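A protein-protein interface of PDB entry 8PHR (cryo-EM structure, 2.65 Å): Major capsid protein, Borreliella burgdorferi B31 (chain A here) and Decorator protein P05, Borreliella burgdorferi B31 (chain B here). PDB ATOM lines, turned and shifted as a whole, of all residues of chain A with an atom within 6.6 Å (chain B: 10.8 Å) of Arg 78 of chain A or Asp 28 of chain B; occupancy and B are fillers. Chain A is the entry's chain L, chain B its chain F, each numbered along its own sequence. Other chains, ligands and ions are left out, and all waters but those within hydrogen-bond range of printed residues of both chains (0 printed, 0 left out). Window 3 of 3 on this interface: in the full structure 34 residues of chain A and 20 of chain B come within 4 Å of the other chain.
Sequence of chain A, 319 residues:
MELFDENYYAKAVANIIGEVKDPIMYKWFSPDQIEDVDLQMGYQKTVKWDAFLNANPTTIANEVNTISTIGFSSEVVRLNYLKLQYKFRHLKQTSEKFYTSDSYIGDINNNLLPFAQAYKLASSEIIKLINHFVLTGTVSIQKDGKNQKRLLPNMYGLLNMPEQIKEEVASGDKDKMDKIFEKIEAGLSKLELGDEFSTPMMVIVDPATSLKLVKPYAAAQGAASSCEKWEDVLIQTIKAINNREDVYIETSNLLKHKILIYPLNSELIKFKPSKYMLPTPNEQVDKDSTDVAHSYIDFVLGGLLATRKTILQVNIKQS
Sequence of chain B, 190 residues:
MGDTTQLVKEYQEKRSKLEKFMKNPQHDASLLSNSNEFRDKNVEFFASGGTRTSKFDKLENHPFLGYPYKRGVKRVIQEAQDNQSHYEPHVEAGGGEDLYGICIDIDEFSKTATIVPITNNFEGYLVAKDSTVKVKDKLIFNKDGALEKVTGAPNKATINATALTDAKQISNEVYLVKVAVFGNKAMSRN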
ATOM      1  N   GLY A  42      -6.629   4.458  26.705  1.00  0.00           N
ATOM      2  CA  GLY A  42      -7.494   5.259  27.546  1.00  0.00           C
ATOM      3  C   GLY A  42      -7.498   6.721  27.159  1.00  0.00           C
ATOM      4  O   GLY A  42      -7.391   7.054  25.977  1.00  0.00           O
ATOM      5  N   TYR A  43      -7.609   7.607  28.145  1.00  0.00           N
ATOM      6  CA  TYR A  43      -7.630   9.036  27.881  1.00  0.00           C
ATOM      7  C   TYR A  43      -6.838   9.766  28.955  1.00  0.00           C
ATOM      8  O   TYR A  43      -6.656   9.272  30.071  1.00  0.00           O
ATOM      9  CB  TYR A  43      -9.072   9.569  27.790  1.00  0.00           C
ATOM     10  CG  TYR A  43      -9.929   9.366  29.027  1.00  0.00           C
ATOM     11  CD1 TYR A  43      -9.713  10.106  30.185  1.00  0.00           C
ATOM     12  CD2 TYR A  43     -10.957   8.432  29.032  1.00  0.00           C
ATOM     13  CE1 TYR A  43     -10.495   9.920  31.309  1.00  0.00           C
ATOM     14  CE2 TYR A  43     -11.743   8.239  30.154  1.00  0.00           C
ATOM     15  CZ  TYR A  43     -11.507   8.985  31.289  1.00  0.00           C
ATOM     16  OH  TYR A  43     -12.286   8.798  32.407  1.00  0.00           O
ATOM     17  N   GLN A  44      -6.364  10.955  28.597  1.00  0.00           N
ATOM     18  CA  GLN A  44      -5.635  11.813  29.519  1.00  0.00           C
ATOM     19  C   GLN A  44      -6.069  13.253  29.296  1.00  0.00           C
ATOM     20  O   GLN A  44      -6.205  13.697  28.154  1.00  0.00           O
ATOM     21  CB  GLN A  44      -4.118  11.680  29.337  1.00  0.00           C
ATOM     22  CG  GLN A  44      -3.304  12.296  30.462  1.00  0.00           C
ATOM     23  CD  GLN A  44      -1.854  11.857  30.443  1.00  0.00           C
ATOM     24  OE1 GLN A  44      -1.443  11.064  29.595  1.00  0.00           O
ATOM     25  NE2 GLN A  44      -1.067  12.371  31.383  1.00  0.00           N
ATOM     26  N   LYS A  45      -6.284  13.977  30.389  1.00  0.00           N
ATOM     27  CA  LYS A  45      -6.799  15.336  30.336  1.00  0.00           C
ATOM     28  C   LYS A  45      -5.707  16.334  30.692  1.00  0.00           C
ATOM     29  O   LYS A  45      -4.904  16.100  31.601  1.00  0.00           O
ATOM     30  CB  LYS A  45      -7.993  15.509  31.279  1.00  0.00           C
ATOM     31  CG  LYS A  45      -9.174  14.616  30.944  1.00  0.00           C
ATOM     32  CD  LYS A  45     -10.398  14.985  31.762  1.00  0.00           C
ATOM     33  CE  LYS A  45     -11.513  13.970  31.569  1.00  0.00           C
ATOM     34  NZ  LYS A  45     -12.790  14.430  32.179  1.00  0.00           N
ATOM     35  N   THR A  46      -5.688  17.449  29.967  1.00  0.00           N
ATOM     36  CA  THR A  46      -4.755  18.540  30.198  1.00  0.00           C
ATOM     37  C   THR A  46      -5.544  19.818  30.437  1.00  0.00           C
ATOM     38  O   THR A  46      -6.550  20.072  29.766  1.00  0.00           O
ATOM     39  CB  THR A  46      -3.797  18.729  29.014  1.00  0.00           C
ATOM     40  OG1 THR A  46      -4.552  18.957  27.817  1.00  0.00           O
ATOM     41  CG2 THR A  46      -2.925  17.495  28.832  1.00  0.00           C
ATOM     42  N   VAL A  76     -10.163  22.470  29.451  1.00  0.00           N
ATOM     43  CA  VAL A  76      -9.804  21.066  29.614  1.00  0.00           C
ATOM     44  C   VAL A  76      -9.839  20.395  28.248  1.00  0.00           C
ATOM     45  O   VAL A  76     -10.811  20.551  27.500  1.00  0.00           O
ATOM     46  CB  VAL A  76     -10.747  20.351  30.599  1.00  0.00           C
ATOM     47  CG1 VAL A  76     -10.364  18.885  30.735  1.00  0.00           C
ATOM     48  CG2 VAL A  76     -10.723  21.043  31.953  1.00  0.00           C
ATOM     49  N   VAL A  77      -8.780  19.653  27.925  1.00  0.00           N
ATOM     50  CA  VAL A  77      -8.663  18.962  26.646  1.00  0.00           C
ATOM     51  C   VAL A  77      -8.343  17.498  26.909  1.00  0.00           C
ATOM     52  O   VAL A  77      -7.421  17.186  27.670  1.00  0.00           O
ATOM     53  CB  VAL A  77      -7.586  19.601  25.748  1.00  0.00           C
ATOM     54  CG1 VAL A  77      -7.195  18.654  24.623  1.00  0.00           C
ATOM     55  CG2 VAL A  77      -8.084  20.923  25.186  1.00  0.00           C
ATOM     56  N   ARG A  78      -9.098  16.602  26.274  1.00  0.00           N
ATOM     57  CA  ARG A  78      -8.911  15.165  26.420  1.00  0.00           C
ATOM     58  C   ARG A  78      -8.192  14.609  25.197  1.00  0.00           C
ATOM     59  O   ARG A  78      -8.543  14.941  24.060  1.00  0.00           O
ATOM     60  CB  ARG A  78     -10.255  14.454  26.600  1.00  0.00           C
ATOM     61  CG  ARG A  78     -10.153  12.935  26.590  1.00  0.00           C
ATOM     62  CD  ARG A  78     -11.520  12.268  26.576  1.00  0.00           C
ATOM     63  NE  ARG A  78     -12.260  12.477  27.816  1.00  0.00           N
ATOM     64  CZ  ARG A  78     -13.474  13.006  27.882  1.00  0.00           C
ATOM     65  NH1 ARG A  78     -14.118  13.395  26.794  1.00  0.00           N
ATOM     66  NH2 ARG A  78     -14.056  13.148  29.069  1.00  0.00           N
ATOM     67  N   LEU A  79      -7.189  13.765  25.434  1.00  0.00           N
ATOM     68  CA  LEU A  79      -6.461  13.076  24.377  1.00  0.00           C
ATOM     69  C   LEU A  79      -6.600  11.575  24.584  1.00  0.00           C
ATOM     70  O   LEU A  79      -6.344  11.071  25.684  1.00  0.00           O
ATOM     71  CB  LEU A  79      -4.985  13.479  24.368  1.00  0.00           C
ATOM     72  CG  LEU A  79      -4.667  14.891  23.872  1.00  0.00           C
ATOM     73  CD1 LEU A  79      -3.167  15.074  23.696  1.00  0.00           C
ATOM     74  CD2 LEU A  79      -5.403  15.186  22.574  1.00  0.00           C
ATOM     75  N   ASN A  80      -7.008  10.868  23.533  1.00  0.00           N
ATOM     76  CA  ASN A  80      -7.235   9.432  23.590  1.00  0.00           C
ATOM     77  C   ASN A  80      -6.029   8.677  23.047  1.00  0.00           C
ATOM     78  O   ASN A  80      -5.384   9.117  22.090  1.00  0.00           O
ATOM     79  CB  ASN A  80      -8.487   9.044  22.799  1.00  0.00           C
ATOM     80  CG  ASN A  80      -9.769   9.481  23.480  1.00  0.00           C
ATOM     81  OD1 ASN A  80      -9.963   9.245  24.672  1.00  0.00           O
ATOM     82  ND2 ASN A  80     -10.656  10.115  22.722  1.00  0.00           N
ATOM     83  N   PRO A 153     -12.665   9.037  18.698  1.00  0.00           N
ATOM     84  CA  PRO A 153     -12.681  10.502  18.680  1.00  0.00           C
ATOM     85  C   PRO A 153     -11.536  11.073  19.503  1.00  0.00           C
ATOM     86  O   PRO A 153     -10.909  10.384  20.312  1.00  0.00           O
ATOM     87  CB  PRO A 153     -14.041  10.859  19.293  1.00  0.00           C
ATOM     88  CG  PRO A 153     -14.858   9.608  19.184  1.00  0.00           C
ATOM     89  CD  PRO A 153     -13.885   8.482  19.307  1.00  0.00           C
ATOM     90  N   ASN A 154     -11.265  12.359  19.271  1.00  0.00           N
ATOM     91  CA  ASN A 154     -10.138  13.064  19.890  1.00  0.00           C
ATOM     92  C   ASN A 154      -8.804  12.423  19.516  1.00  0.00           C
ATOM     93  O   ASN A 154      -7.823  12.524  20.256  1.00  0.00           O
ATOM     94  CB  ASN A 154     -10.289  13.140  21.414  1.00  0.00           C
ATOM     95  CG  ASN A 154     -11.425  14.045  21.844  1.00  0.00           C
ATOM     96  OD1 ASN A 154     -12.576  13.844  21.457  1.00  0.00           O
ATOM     97  ND2 ASN A 154     -11.108  15.046  22.655  1.00  0.00           N
ATOM     98  N   MET A 155      -8.764  11.762  18.359  1.00  0.00           N
ATOM     99  CA  MET A 155      -7.558  11.136  17.821  1.00  0.00           C
ATOM    100  C   MET A 155      -7.392  11.676  16.404  1.00  0.00           C
ATOM    101  O   MET A 155      -7.950  11.125  15.452  1.00  0.00           O
ATOM    102  CB  MET A 155      -7.663   9.614  17.842  1.00  0.00           C
ATOM    103  CG  MET A 155      -7.057   8.958  19.069  1.00  0.00           C
ATOM    104  SD  MET A 155      -7.190   7.160  19.009  1.00  0.00           S
ATOM    105  CE  MET A 155      -5.571   6.718  18.387  1.00  0.00           C
ATOM    106  N   TYR B  11     -29.919  12.944  24.496  1.00  0.00           N
ATOM    107  CA  TYR B  11     -28.993  13.178  25.598  1.00  0.00           C
ATOM    108  C   TYR B  11     -28.138  14.412  25.345  1.00  0.00           C
ATOM    109  O   TYR B  11     -27.951  15.239  26.244  1.00  0.00           O
ATOM    110  CB  TYR B  11     -28.111  11.948  25.811  1.00  0.00           C
ATOM    111  CG  TYR B  11     -27.124  12.086  26.948  1.00  0.00           C
ATOM    112  CD1 TYR B  11     -27.540  12.006  28.271  1.00  0.00           C
ATOM    113  CD2 TYR B  11     -25.775  12.299  26.697  1.00  0.00           C
ATOM    114  CE1 TYR B  11     -26.640  12.132  29.312  1.00  0.00           C
ATOM    115  CE2 TYR B  11     -24.867  12.426  27.732  1.00  0.00           C
ATOM    116  CZ  TYR B  11     -25.304  12.341  29.036  1.00  0.00           C
ATOM    117  OH  TYR B  11     -24.402  12.468  30.067  1.00  0.00           O
ATOM    118  N   ARG B  15     -28.341  17.734  27.653  1.00  0.00           N
ATOM    119  CA  ARG B  15     -27.123  18.165  28.326  1.00  0.00           C
ATOM    120  C   ARG B  15     -26.757  19.592  27.945  1.00  0.00           C
ATOM    121  O   ARG B  15     -26.368  20.390  28.805  1.00  0.00           O
ATOM    122  CB  ARG B  15     -25.973  17.212  27.998  1.00  0.00           C
ATOM    123  CG  ARG B  15     -24.684  17.532  28.735  1.00  0.00           C
ATOM    124  CD  ARG B  15     -23.544  16.638  28.284  1.00  0.00           C
ATOM    125  NE  ARG B  15     -22.322  16.899  29.036  1.00  0.00           N
ATOM    126  CZ  ARG B  15     -21.177  16.260  28.851  1.00  0.00           C
ATOM    127  NH1 ARG B  15     -21.056  15.305  27.944  1.00  0.00           N
ATOM    128  NH2 ARG B  15     -20.124  16.586  29.595  1.00  0.00           N
ATOM    129  N   GLU B  19     -26.616  22.615  30.629  1.00  0.00           N
ATOM    130  CA  GLU B  19     -25.350  23.300  30.840  1.00  0.00           C
ATOM    131  C   GLU B  19     -25.360  24.737  30.336  1.00  0.00           C
ATOM    132  O   GLU B  19     -24.442  25.496  30.666  1.00  0.00           O
ATOM    133  CB  GLU B  19     -24.217  22.520  30.168  1.00  0.00           C
ATOM    134  CG  GLU B  19     -23.613  21.440  31.054  1.00  0.00           C
ATOM    135  CD  GLU B  19     -22.871  20.380  30.263  1.00  0.00           C
ATOM    136  OE1 GLU B  19     -22.957  20.395  29.018  1.00  0.00           O
ATOM    137  OE2 GLU B  19     -22.201  19.532  30.888  1.00  0.00           O
ATOM    138  N   ASN B  24     -20.035  27.608  35.199  1.00  0.00           N
ATOM    139  CA  ASN B  24     -18.831  27.030  34.605  1.00  0.00           C
ATOM    140  C   ASN B  24     -19.110  25.587  34.204  1.00  0.00           C
ATOM    141  O   ASN B  24     -18.645  24.646  34.858  1.00  0.00           O
ATOM    142  CB  ASN B  24     -17.650  27.115  35.574  1.00  0.00           C
ATOM    143  CG  ASN B  24     -16.324  26.806  34.909  1.00  0.00           C
ATOM    144  OD1 ASN B  24     -16.249  26.654  33.689  1.00  0.00           O
ATOM    145  ND2 ASN B  24     -15.268  26.713  35.708  1.00  0.00           N
ATOM    146  N   PRO B  25     -19.882  25.377  33.138  1.00  0.00           N
ATOM    147  CA  PRO B  25     -20.132  24.007  32.676  1.00  0.00           C
ATOM    148  C   PRO B  25     -18.843  23.340  32.217  1.00  0.00           C
ATOM    149  O   PRO B  25     -17.962  23.981  31.640  1.00  0.00           O
ATOM    150  CB  PRO B  25     -21.118  24.196  31.517  1.00  0.00           C
ATOM    151  CG  PRO B  25     -20.893  25.592  31.051  1.00  0.00           C
ATOM    152  CD  PRO B  25     -20.517  26.383  32.268  1.00  0.00           C
ATOM    153  N   GLN B  26     -18.741  22.040  32.479  1.00  0.00           N
ATOM    154  CA  GLN B  26     -17.539  21.273  32.156  1.00  0.00           C
ATOM    155  C   GLN B  26     -17.724  20.650  30.778  1.00  0.00           C
ATOM    156  O   GLN B  26     -18.369  19.610  30.633  1.00  0.00           O
ATOM    157  CB  GLN B  26     -17.275  20.217  33.224  1.00  0.00           C
ATOM    158  CG  GLN B  26     -15.904  19.563  33.137  1.00  0.00           C
ATOM    159  CD  GLN B  26     -15.887  18.348  32.229  1.00  0.00           C
ATOM    160  OE1 GLN B  26     -16.884  17.636  32.108  1.00  0.00           O
ATOM    161  NE2 GLN B  26     -14.750  18.104  31.589  1.00  0.00           N
ATOM    162  N   HIS B  27     -17.157  21.293  29.760  1.00  0.00           N
ATOM    163  CA  HIS B  27     -17.212  20.814  28.382  1.00  0.00           C
ATOM    164  C   HIS B  27     -15.798  20.475  27.932  1.00  0.00           C
ATOM    165  O   HIS B  27     -14.977  21.374  27.723  1.00  0.00           O
ATOM    166  CB  HIS B  27     -17.837  21.858  27.456  1.00  0.00           C
ATOM    167  CG  HIS B  27     -19.289  22.109  27.715  1.00  0.00           C
ATOM    168  ND1 HIS B  27     -20.245  22.024  26.726  1.00  0.00           N
ATOM    169  CD2 HIS B  27     -19.949  22.444  28.848  1.00  0.00           C
ATOM    170  CE1 HIS B  27     -21.431  22.298  27.238  1.00  0.00           C
ATOM    171  NE2 HIS B  27     -21.281  22.554  28.525  1.00  0.00           N
ATOM    172  N   ASP B  28     -15.514  19.184  27.787  1.00  0.00           N
ATOM    173  CA  ASP B  28     -14.222  18.764  27.265  1.00  0.00           C
ATOM    174  C   ASP B  28     -14.115  19.108  25.784  1.00  0.00           C
ATOM    175  O   ASP B  28     -15.059  18.914  25.013  1.00  0.00           O
ATOM    176  CB  ASP B  28     -14.023  17.264  27.478  1.00  0.00           C
ATOM    177  CG  ASP B  28     -13.516  16.938  28.868  1.00  0.00           C
ATOM    178  OD1 ASP B  28     -13.353  17.876  29.677  1.00  0.00           O
ATOM    179  OD2 ASP B  28     -13.277  15.746  29.153  1.00  0.00           O
ATOM    180  N   ALA B  29     -12.955  19.623  25.389  1.00  0.00           N
ATOM    181  CA  ALA B  29     -12.709  20.047  24.019  1.00  0.00           C
ATOM    182  C   ALA B  29     -11.579  19.222  23.421  1.00  0.00           C
ATOM    183  O   ALA B  29     -10.621  18.866  24.114  1.00  0.00           O
ATOM    184  CB  ALA B  29     -12.361  21.538  23.952  1.00  0.00           C
ATOM    185  N   SER B  30     -11.699  18.918  22.127  1.00  0.00           N
ATOM    186  CA  SER B  30     -10.676  18.131  21.451  1.00  0.00           C
ATOM    187  C   SER B  30      -9.403  18.927  21.195  1.00  0.00           C
ATOM    188  O   SER B  30      -8.348  18.326  20.967  1.00  0.00           O
ATOM    189  CB  SER B  30     -11.222  17.583  20.132  1.00  0.00           C
ATOM    190  OG  SER B  30     -11.679  18.630  19.294  1.00  0.00           O
ATOM    191  N   LEU B  31      -9.477  20.256  21.224  1.00  0.00           N
ATOM    192  CA  LEU B  31      -8.331  21.100  20.921  1.00  0.00           C
ATOM    193  C   LEU B  31      -8.402  22.375  21.748  1.00  0.00           C
ATOM    194  O   LEU B  31      -9.478  22.792  22.187  1.00  0.00           O
ATOM    195  CB  LEU B  31      -8.263  21.441  19.424  1.00  0.00           C
ATOM    196  CG  LEU B  31      -9.240  22.465  18.837  1.00  0.00           C
ATOM    197  CD1 LEU B  31      -8.839  22.789  17.410  1.00  0.00           C
ATOM    198  CD2 LEU B  31     -10.681  21.980  18.880  1.00  0.00           C
ATOM    199  N   LEU B  32      -7.241  22.990  21.956  1.00  0.00           N
ATOM    200  CA  LEU B  32      -7.158  24.214  22.737  1.00  0.00           C
ATOM    201  C   LEU B  32      -7.672  25.407  21.936  1.00  0.00           C
ATOM    202  O   LEU B  32      -7.756  25.381  20.705  1.00  0.00           O
ATOM    203  CB  LEU B  32      -5.719  24.471  23.183  1.00  0.00           C
ATOM    204  CG  LEU B  32      -5.144  23.539  24.250  1.00  0.00           C
ATOM    205  CD1 LEU B  32      -3.639  23.722  24.357  1.00  0.00           C
ATOM    206  CD2 LEU B  32      -5.812  23.792  25.591  1.00  0.00           C
ATOM    207  N   SER B  33      -8.018  26.467  22.661  1.00  0.00           N
ATOM    208  CA  SER B  33      -8.481  27.713  22.074  1.00  0.00           C
ATOM    209  C   SER B  33      -7.400  28.779  22.197  1.00  0.00           C
ATOM    210  O   SER B  33      -6.575  28.748  23.114  1.00  0.00           O
ATOM    211  CB  SER B  33      -9.768  28.197  22.750  1.00  0.00           C
ATOM    212  OG  SER B  33      -9.488  28.825  23.988  1.00  0.00           O
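The side-chain amino group (NZ) of Lys 45 of chain A is in salt-bridge range of the side-chain carboxylate (OD2) of Asp 28 of chain B (3.3 Å). The backbone NH (N) of Ala 29 of chain B is in hydrogen-bond range of the backbone carbonyl oxygen (O) of Val 76 of chain A (3.1 Å). The side-chain carboxylate of Asp 28 of chain B is in salt-bridge range of the guanidinium group of Arg 78 of chain A (2.7 Å). O of Ala 29 of chain B lies within hydrogen-bond range of N of Arg 78 of chain A, 3.5 Å away.
The backbone NH of Thr 46 of chain A sits at hydrogen-bond distance from the backbone carbonyl oxygen of Val 77 of chain A (2.9 Å). O of Arg 78 of chain A sits at hydrogen-bond distance from ND2 of Asn 154 of chain A, at 2.9 Å.
Among the printed residues, pairs that only touch across the chains: Val 77 of chain A with Ala 29 of chain B, Val 76 of chain A with Asp 28 of chain B, Asn 154 of chain A with Ser 30 of chain B, Val 77 of chain A with Leu 32 of chain B, Val 77 of chain A with Leu 31 of chain B and Val 77 of chain A with Ser 30 of chain B.
Of the printed residues of chain B, Lys 45 of chain A touches Asp 28 (3.3 Å). Thr 46 of chain A touches none of the printed residues of chain B. Of chain B, only Asp 28 (3.3 Å) and Ala 29 (3.1 Å) come within 4 Å of Val 76 of chain A. Printed residues of chain B within 4 Å of Val 77 of chain A: Ala 29 (3.2 Å), Ser 30 (3.8 Å), Leu 31 (3.7 Å) and Leu 32 (3.7 Å). No residue of chain B comes within 4 Å of Leu 79 of chain A. Printed residues of chain A within 4 Å of Leu 32 of chain B: Val 77. Of the printed residues of chain A, Leu 31 of chain B touches Val 77 (3.7 Å). Of the printed residues of chain A, Ala 29 of chain B touches Val 76 (3.1 Å), Val 77 (3.2 Å) and Arg 78 (3.5 Å). Printed residues of chain A within 4 Å of Ser 30 of chain B: Val 77 (3.8 Å) and Asn 154 (3.3 Å). The nearest residue of chain B that does not touch Arg 78 of chain A is Ser 30 of chain B (4.6 Å).
Printed residues of chain A that touch a printed residue of chain B: Lys 45, Val 76, Val 77, Arg 78 and Asn 154. Hydrophobic or aromatic side chains of chain A within 4 Å of the printed part of chain B: Val 76 and Val 77. Of the 13 printed residues of chain B, 5 touch a printed residue of chain A. Among the printed residues, 10 pairs touch across the chains. Among the printed residues, Asp or Glu carboxylates within 4 Å of a Lys or Arg side-chain nitrogen of the other chain: Lys 45 of chain A with Asp 28 of chain B and Arg 78 of chain A with Asp 28 of chain B.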
